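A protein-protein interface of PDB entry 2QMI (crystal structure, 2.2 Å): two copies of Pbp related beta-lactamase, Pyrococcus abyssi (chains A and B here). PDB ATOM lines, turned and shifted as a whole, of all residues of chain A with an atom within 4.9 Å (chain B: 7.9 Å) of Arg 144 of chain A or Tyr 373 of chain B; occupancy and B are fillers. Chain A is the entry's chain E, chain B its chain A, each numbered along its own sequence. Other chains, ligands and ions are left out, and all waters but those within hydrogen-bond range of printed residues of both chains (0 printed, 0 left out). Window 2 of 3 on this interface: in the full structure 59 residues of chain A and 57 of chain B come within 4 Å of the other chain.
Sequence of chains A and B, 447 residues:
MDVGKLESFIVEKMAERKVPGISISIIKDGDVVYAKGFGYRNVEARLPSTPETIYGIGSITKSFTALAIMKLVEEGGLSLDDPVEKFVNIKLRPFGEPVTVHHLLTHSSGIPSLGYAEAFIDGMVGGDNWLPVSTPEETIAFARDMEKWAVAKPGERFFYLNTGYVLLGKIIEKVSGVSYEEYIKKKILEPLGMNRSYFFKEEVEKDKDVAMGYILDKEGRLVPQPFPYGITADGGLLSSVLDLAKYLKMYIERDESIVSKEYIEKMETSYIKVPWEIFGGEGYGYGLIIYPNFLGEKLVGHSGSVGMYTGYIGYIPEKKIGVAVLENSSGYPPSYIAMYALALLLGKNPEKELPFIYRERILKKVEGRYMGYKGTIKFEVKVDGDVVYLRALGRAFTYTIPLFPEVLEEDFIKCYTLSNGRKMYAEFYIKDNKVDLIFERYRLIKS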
ATOM      1  N   ILE A  90     -11.914  27.690  28.997  1.00  0.00           N
ATOM      2  CA  ILE A  90     -11.786  26.674  27.952  1.00  0.00           C
ATOM      3  C   ILE A  90     -12.040  25.290  28.562  1.00  0.00           C
ATOM      4  O   ILE A  90     -11.770  25.074  29.747  1.00  0.00           O
ATOM      5  CB  ILE A  90     -10.363  26.722  27.343  1.00  0.00           C
ATOM      6  CG1 ILE A  90     -10.277  25.839  26.099  1.00  0.00           C
ATOM      7  CG2 ILE A  90      -9.331  26.269  28.382  1.00  0.00           C
ATOM      8  CD1 ILE A  90      -8.947  25.957  25.361  1.00  0.00           C
ATOM      9  N   LEU A 114      -0.922  20.335  18.457  1.00  0.00           N
ATOM     10  CA  LEU A 114      -1.956  20.832  17.557  1.00  0.00           C
ATOM     11  C   LEU A 114      -1.334  21.311  16.246  1.00  0.00           C
ATOM     12  O   LEU A 114      -2.044  21.642  15.296  1.00  0.00           O
ATOM     13  CB  LEU A 114      -2.716  21.988  18.213  1.00  0.00           C
ATOM     14  CG  LEU A 114      -3.474  21.722  19.512  1.00  0.00           C
ATOM     15  CD1 LEU A 114      -4.214  22.990  19.931  1.00  0.00           C
ATOM     16  CD2 LEU A 114      -4.456  20.574  19.315  1.00  0.00           C
ATOM     17  N   ILE A 140      -5.709  30.624  21.394  1.00  0.00           N
ATOM     18  CA  ILE A 140      -6.550  29.953  22.379  1.00  0.00           C
ATOM     19  C   ILE A 140      -7.940  29.687  21.811  1.00  0.00           C
ATOM     20  O   ILE A 140      -8.500  28.609  22.007  1.00  0.00           O
ATOM     21  CB  ILE A 140      -6.631  30.782  23.687  1.00  0.00           C
ATOM     22  CG1 ILE A 140      -5.273  30.739  24.398  1.00  0.00           C
ATOM     23  CG2 ILE A 140      -7.718  30.234  24.593  1.00  0.00           C
ATOM     24  CD1 ILE A 140      -5.158  31.645  25.614  1.00  0.00           C
ATOM     25  N   ALA A 141      -8.492  30.666  21.100  1.00  0.00           N
ATOM     26  CA  ALA A 141      -9.802  30.501  20.478  1.00  0.00           C
ATOM     27  C   ALA A 141      -9.721  29.335  19.482  1.00  0.00           C
ATOM     28  O   ALA A 141     -10.610  28.491  19.419  1.00  0.00           O
ATOM     29  CB  ALA A 141     -10.211  31.796  19.760  1.00  0.00           C
ATOM     30  N   PHE A 142      -8.638  29.291  18.712  1.00  0.00           N
ATOM     31  CA  PHE A 142      -8.419  28.222  17.747  1.00  0.00           C
ATOM     32  C   PHE A 142      -8.335  26.887  18.478  1.00  0.00           C
ATOM     33  O   PHE A 142      -8.821  25.876  17.982  1.00  0.00           O
ATOM     34  CB  PHE A 142      -7.111  28.459  16.981  1.00  0.00           C
ATOM     35  CG  PHE A 142      -6.744  27.349  16.021  1.00  0.00           C
ATOM     36  CD1 PHE A 142      -7.501  27.114  14.875  1.00  0.00           C
ATOM     37  CD2 PHE A 142      -5.632  26.549  16.258  1.00  0.00           C
ATOM     38  CE1 PHE A 142      -7.151  26.094  13.977  1.00  0.00           C
ATOM     39  CE2 PHE A 142      -5.272  25.530  15.368  1.00  0.00           C
ATOM     40  CZ  PHE A 142      -6.034  25.303  14.226  1.00  0.00           C
ATOM     41  N   ALA A 143      -7.725  26.898  19.664  1.00  0.00           N
ATOM     42  CA  ALA A 143      -7.545  25.686  20.464  1.00  0.00           C
ATOM     43  C   ALA A 143      -8.790  25.256  21.243  1.00  0.00           C
ATOM     44  O   ALA A 143      -8.740  24.306  22.031  1.00  0.00           O
ATOM     45  CB  ALA A 143      -6.380  25.879  21.431  1.00  0.00           C
ATOM     46  N   ARG A 144      -9.896  25.958  21.009  1.00  0.00           N
ATOM     47  CA  ARG A 144     -11.165  25.698  21.682  1.00  0.00           C
ATOM     48  C   ARG A 144     -11.606  24.233  21.785  1.00  0.00           C
ATOM     49  O   ARG A 144     -12.230  23.853  22.772  1.00  0.00           O
ATOM     50  CB  ARG A 144     -12.261  26.546  21.019  1.00  0.00           C
ATOM     51  CG  ARG A 144     -13.699  26.196  21.381  1.00  0.00           C
ATOM     52  CD  ARG A 144     -14.647  27.311  20.918  1.00  0.00           C
ATOM     53  NE  ARG A 144     -16.013  26.847  20.669  1.00  0.00           N
ATOM     54  CZ  ARG A 144     -16.383  26.152  19.596  1.00  0.00           C
ATOM     55  NH1 ARG A 144     -17.648  25.771  19.458  1.00  0.00           N
ATOM     56  NH2 ARG A 144     -15.493  25.842  18.659  1.00  0.00           N
ATOM     57  N   ASP A 145     -11.292  23.410  20.789  1.00  0.00           N
ATOM     58  CA  ASP A 145     -11.688  21.997  20.834  1.00  0.00           C
ATOM     59  C   ASP A 145     -10.555  21.050  21.215  1.00  0.00           C
ATOM     60  O   ASP A 145     -10.691  19.832  21.073  1.00  0.00           O
ATOM     61  CB  ASP A 145     -12.241  21.549  19.481  1.00  0.00           C
ATOM     62  CG  ASP A 145     -13.406  22.389  19.023  1.00  0.00           C
ATOM     63  OD1 ASP A 145     -14.302  22.665  19.850  1.00  0.00           O
ATOM     64  OD2 ASP A 145     -13.430  22.762  17.832  1.00  0.00           O
ATOM     65  N   MET A 146      -9.444  21.592  21.710  1.00  0.00           N
ATOM     66  CA  MET A 146      -8.311  20.744  22.046  1.00  0.00           C
ATOM     67  C   MET A 146      -8.616  19.573  22.977  1.00  0.00           C
ATOM     68  O   MET A 146      -7.967  18.531  22.876  1.00  0.00           O
ATOM     69  CB  MET A 146      -7.147  21.579  22.594  1.00  0.00           C
ATOM     70  CG  MET A 146      -7.381  22.286  23.910  1.00  0.00           C
ATOM     71  SD  MET A 146      -6.025  23.444  24.232  1.00  0.00           S
ATOM     72  CE  MET A 146      -4.705  22.301  24.617  1.00  0.00           C
ATOM     73  N   TRP A 149      -9.093  16.462  21.303  1.00  0.00           N
ATOM     74  CA  TRP A 149      -7.892  15.972  20.624  1.00  0.00           C
ATOM     75  C   TRP A 149      -7.065  14.986  21.471  1.00  0.00           C
ATOM     76  O   TRP A 149      -6.186  14.299  20.953  1.00  0.00           O
ATOM     77  CB  TRP A 149      -7.028  17.177  20.229  1.00  0.00           C
ATOM     78  CG  TRP A 149      -5.954  16.907  19.211  1.00  0.00           C
ATOM     79  CD1 TRP A 149      -4.612  17.114  19.362  1.00  0.00           C
ATOM     80  CD2 TRP A 149      -6.141  16.466  17.862  1.00  0.00           C
ATOM     81  NE1 TRP A 149      -3.952  16.838  18.186  1.00  0.00           N
ATOM     82  CE2 TRP A 149      -4.868  16.437  17.250  1.00  0.00           C
ATOM     83  CE3 TRP A 149      -7.263  16.094  17.107  1.00  0.00           C
ATOM     84  CZ2 TRP A 149      -4.685  16.051  15.920  1.00  0.00           C
ATOM     85  CZ3 TRP A 149      -7.078  15.710  15.781  1.00  0.00           C
ATOM     86  CH2 TRP A 149      -5.799  15.694  15.205  1.00  0.00           C
ATOM     87  N   MET B 371      -4.079  14.481   8.382  1.00  0.00           N
ATOM     88  CA  MET B 371      -4.191  15.877   8.826  1.00  0.00           C
ATOM     89  C   MET B 371      -4.041  16.049  10.334  1.00  0.00           C
ATOM     90  O   MET B 371      -4.438  15.186  11.120  1.00  0.00           O
ATOM     91  CB  MET B 371      -5.547  16.473   8.430  1.00  0.00           C
ATOM     92  CG  MET B 371      -5.859  16.413   6.968  1.00  0.00           C
ATOM     93  SD  MET B 371      -4.517  17.115   6.028  1.00  0.00           S
ATOM     94  CE  MET B 371      -4.936  18.883   6.116  1.00  0.00           C
ATOM     95  N   GLY B 372      -3.486  17.189  10.730  1.00  0.00           N
ATOM     96  CA  GLY B 372      -3.327  17.472  12.140  1.00  0.00           C
ATOM     97  C   GLY B 372      -4.609  18.100  12.658  1.00  0.00           C
ATOM     98  O   GLY B 372      -5.636  18.087  11.969  1.00  0.00           O
ATOM     99  N   TYR B 373      -4.549  18.646  13.869  1.00  0.00           N
ATOM    100  CA  TYR B 373      -5.702  19.296  14.492  1.00  0.00           C
ATOM    101  C   TYR B 373      -6.288  20.338  13.536  1.00  0.00           C
ATOM    102  O   TYR B 373      -5.611  21.295  13.147  1.00  0.00           O
ATOM    103  CB  TYR B 373      -5.269  19.963  15.800  1.00  0.00           C
ATOM    104  CG  TYR B 373      -6.323  20.817  16.471  1.00  0.00           C
ATOM    105  CD1 TYR B 373      -7.281  20.251  17.309  1.00  0.00           C
ATOM    106  CD2 TYR B 373      -6.330  22.204  16.304  1.00  0.00           C
ATOM    107  CE1 TYR B 373      -8.218  21.046  17.976  1.00  0.00           C
ATOM    108  CE2 TYR B 373      -7.264  23.008  16.961  1.00  0.00           C
ATOM    109  CZ  TYR B 373      -8.199  22.426  17.796  1.00  0.00           C
ATOM    110  OH  TYR B 373      -9.099  23.220  18.466  1.00  0.00           O
ATOM    111  N   LYS B 374      -7.545  20.139  13.154  1.00  0.00           N
ATOM    112  CA  LYS B 374      -8.223  21.052  12.242  1.00  0.00           C
ATOM    113  C   LYS B 374      -7.380  21.426  11.016  1.00  0.00           C
ATOM    114  O   LYS B 374      -7.349  22.588  10.596  1.00  0.00           O
ATOM    115  CB  LYS B 374      -8.655  22.313  13.000  1.00  0.00           C
ATOM    116  CG  LYS B 374      -9.694  22.022  14.079  1.00  0.00           C
ATOM    117  CD  LYS B 374     -10.174  23.274  14.796  1.00  0.00           C
ATOM    118  CE  LYS B 374     -11.154  22.917  15.914  1.00  0.00           C
ATOM    119  NZ  LYS B 374     -12.364  22.191  15.425  1.00  0.00           N
ATOM    120  N   GLY B 375      -6.685  20.434  10.460  1.00  0.00           N
ATOM    121  CA  GLY B 375      -5.876  20.642   9.267  1.00  0.00           C
ATOM    122  C   GLY B 375      -4.653  21.550   9.308  1.00  0.00           C
ATOM    123  O   GLY B 375      -4.292  22.128   8.282  1.00  0.00           O
ATOM    124  N   THR B 376      -3.998  21.668  10.460  1.00  0.00           N
ATOM    125  CA  THR B 376      -2.810  22.514  10.554  1.00  0.00           C
ATOM    126  C   THR B 376      -1.646  21.988   9.713  1.00  0.00           C
ATOM    127  O   THR B 376      -1.065  22.724   8.912  1.00  0.00           O
ATOM    128  CB  THR B 376      -2.320  22.651  12.005  1.00  0.00           C
ATOM    129  OG1 THR B 376      -2.209  21.351  12.594  1.00  0.00           O
ATOM    130  CG2 THR B 376      -3.277  23.517  12.812  1.00  0.00           C
ATOM    131  N   ILE B 377      -1.292  20.722   9.911  1.00  0.00           N
ATOM    132  CA  ILE B 377      -0.198  20.120   9.152  1.00  0.00           C
ATOM    133  C   ILE B 377      -0.702  18.942   8.338  1.00  0.00           C
ATOM    134  O   ILE B 377      -1.620  18.230   8.759  1.00  0.00           O
ATOM    135  CB  ILE B 377       0.952  19.661  10.076  1.00  0.00           C
ATOM    136  CG1 ILE B 377       0.412  18.771  11.201  1.00  0.00           C
ATOM    137  CG2 ILE B 377       1.672  20.880  10.642  1.00  0.00           C
ATOM    138  CD1 ILE B 377       1.479  18.304  12.162  1.00  0.00           C
ATOM    139  N   TYR B 442       3.185  14.536  17.510  1.00  0.00           N
ATOM    140  CA  TYR B 442       1.941  14.742  16.774  1.00  0.00           C
ATOM    141  C   TYR B 442       0.891  13.633  16.761  1.00  0.00           C
ATOM    142  O   TYR B 442       1.157  12.480  17.090  1.00  0.00           O
ATOM    143  CB  TYR B 442       2.271  15.074  15.319  1.00  0.00           C
ATOM    144  CG  TYR B 442       3.327  16.145  15.120  1.00  0.00           C
ATOM    145  CD1 TYR B 442       3.012  17.496  15.240  1.00  0.00           C
ATOM    146  CD2 TYR B 442       4.633  15.801  14.763  1.00  0.00           C
ATOM    147  CE1 TYR B 442       3.963  18.480  15.003  1.00  0.00           C
ATOM    148  CE2 TYR B 442       5.600  16.787  14.523  1.00  0.00           C
ATOM    149  CZ  TYR B 442       5.253  18.121  14.644  1.00  0.00           C
ATOM    150  OH  TYR B 442       6.189  19.096  14.392  1.00  0.00           O
ATOM    151  N   ARG B 443      -0.318  14.031  16.377  1.00  0.00           N
ATOM    152  CA  ARG B 443      -1.445  13.127  16.191  1.00  0.00           C
ATOM    153  C   ARG B 443      -1.942  13.527  14.802  1.00  0.00           C
ATOM    154  O   ARG B 443      -2.126  14.714  14.532  1.00  0.00           O
ATOM    155  CB  ARG B 443      -2.571  13.349  17.207  1.00  0.00           C
ATOM    156  CG  ARG B 443      -3.817  12.525  16.840  1.00  0.00           C
ATOM    157  CD  ARG B 443      -4.993  12.696  17.798  1.00  0.00           C
ATOM    158  NE  ARG B 443      -6.110  11.832  17.414  1.00  0.00           N
ATOM    159  CZ  ARG B 443      -7.260  11.736  18.078  1.00  0.00           C
ATOM    160  NH1 ARG B 443      -7.467  12.450  19.174  1.00  0.00           N
ATOM    161  NH2 ARG B 443      -8.206  10.915  17.649  1.00  0.00           N
ATOM    162  N   LEU B 444      -2.142  12.547  13.932  1.00  0.00           N
ATOM    163  CA  LEU B 444      -2.598  12.802  12.567  1.00  0.00           C
ATOM    164  C   LEU B 444      -3.726  11.831  12.202  1.00  0.00           C
ATOM    165  O   LEU B 444      -3.686  10.657  12.567  1.00  0.00           O
ATOM    166  CB  LEU B 444      -1.424  12.633  11.598  1.00  0.00           C
ATOM    167  CG  LEU B 444      -0.209  13.520  11.893  1.00  0.00           C
ATOM    168  CD1 LEU B 444       1.009  13.016  11.136  1.00  0.00           C
ATOM    169  CD2 LEU B 444      -0.531  14.958  11.519  1.00  0.00           C
ATOM    170  N   ILE B 445      -4.727  12.318  11.477  1.00  0.00           N
ATOM    171  CA  ILE B 445      -5.852  11.469  11.109  1.00  0.00           C
ATOM    172  C   ILE B 445      -6.060  11.411   9.601  1.00  0.00           C
ATOM    173  O   ILE B 445      -6.301  12.435   8.953  1.00  0.00           O
ATOM    174  CB  ILE B 445      -7.148  11.961  11.780  1.00  0.00           C
ATOM    175  CG1 ILE B 445      -6.942  12.042  13.297  1.00  0.00           C
ATOM    176  CG2 ILE B 445      -8.312  11.018  11.431  1.00  0.00           C
ATOM    177  CD1 ILE B 445      -8.106  12.682  14.040  1.00  0.00           C
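No position is printed for both chains.
Of the 13 pairs that touch across the chains among the printed residues, none has its exchanged pair printed and touching as well.
The side-chain hydroxyl (OH) of Tyr 373 of chain B sits at hydrogen-bond distance from the backbone carbonyl oxygen (O) of Phe 142 of chain A, at 2.7 Å.
OH of Tyr 373 of chain B lies within hydrogen-bond range of N of Asp 145 of chain A.
NZ of Lys 374 of chain B lies within salt-bridge range of OD2 of Asp 145 of chain A.
OG1 of Thr 376 of chain B is in hydrogen-bond range of O of Leu 114 of chain A.
The guanidinium group of Arg 443 of chain B sits at hydrogen-bond distance from the backbone carbonyl oxygen of Trp 149 of chain A (2.9 Å).
Printed residues of chain B within 4 Å of Phe 142 of chain A: Tyr 373 (2.7 Å) and Thr 376 (3.6 Å).
Of the printed residues of chain B, Ala 143 of chain A touches Tyr 373.
Of chain B, only Tyr 373 comes within 4 Å of Arg 144 of chain A.
Met 371 of chain B touches none of the printed residues of chain A.
Tyr 373 of chain B touches seven residues of chain A.
Of the printed residues of chain A, Thr 376 of chain B touches Leu 114 and Phe 142.
Printed residues of chain A within 4 Å of Arg 443 of chain B: Trp 149 (2.9 Å).
Printed residues of chain A within 4 Å of Ile 445 of chain B: Trp 149 (3.6 Å).
The nearest residue of chain B that does not touch Arg 144 of chain A is Lys 374 of chain B (5.8 Å).
The nearest printed residue of chain A that does not touch Tyr 373 of chain B is Ala 141 of chain A (5.6 Å).
The nearest printed residue of chain B that does not touch Asp 145 of chain A is Arg 443 of chain B (8.3 Å).
Printed residues of chain B that touch a printed residue of chain A: Gly 372, Tyr 373, Lys 374, Thr 376, Arg 443 and Ile 445.
Hydrophobic or aromatic side chains of chain B within 4 Å of the printed part of chain A: Tyr 373 and Ile 445.
Of the 10 printed residues of chain A, 7 touch a printed residue of chain B.
Hydrophobic or aromatic side chains of chain A within 4 Å of the printed part of chain B: Leu 114, Phe 142 and Trp 149.
Among the printed residues, pairs that only touch across the chains: Trp 149 of chain A with Tyr 373 of chain B (3.3 Å), Leu 114 of chain A with Tyr 373 of chain B (3.4 Å), Ala 143 of chain A with Tyr 373 of chain B (3.5 Å), Phe 142 of chain A with Thr 376 of chain B (3.6 Å), Trp 149 of chain A with Ile 445 of chain B (3.6 Å), Met 146 of chain A with Tyr 373 of chain B (3.6 Å), Trp 149 of chain A with Gly 372 of chain B (3.7 Å) and Arg 144 of chain A with Tyr 373 of chain B (3.8 Å).
The backbone carbonyl oxygen of Met 371 of chain B sits at hydrogen-bond distance from the backbone NH of Ile 445 of chain B (2.9 Å).
The backbone NH of Gly 372 of chain B lies within hydrogen-bond range of the backbone carbonyl oxygen of Ile 377 of chain B (2.9 Å).
O of Tyr 373 of chain B lies close to OG1 of Thr 376 of chain B.
The side-chain carboxylate (OD1) of Asp 145 of chain A is in salt-bridge range of the guanidinium group (NH2) of Arg 144 of chain A, 3.6 Å away.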
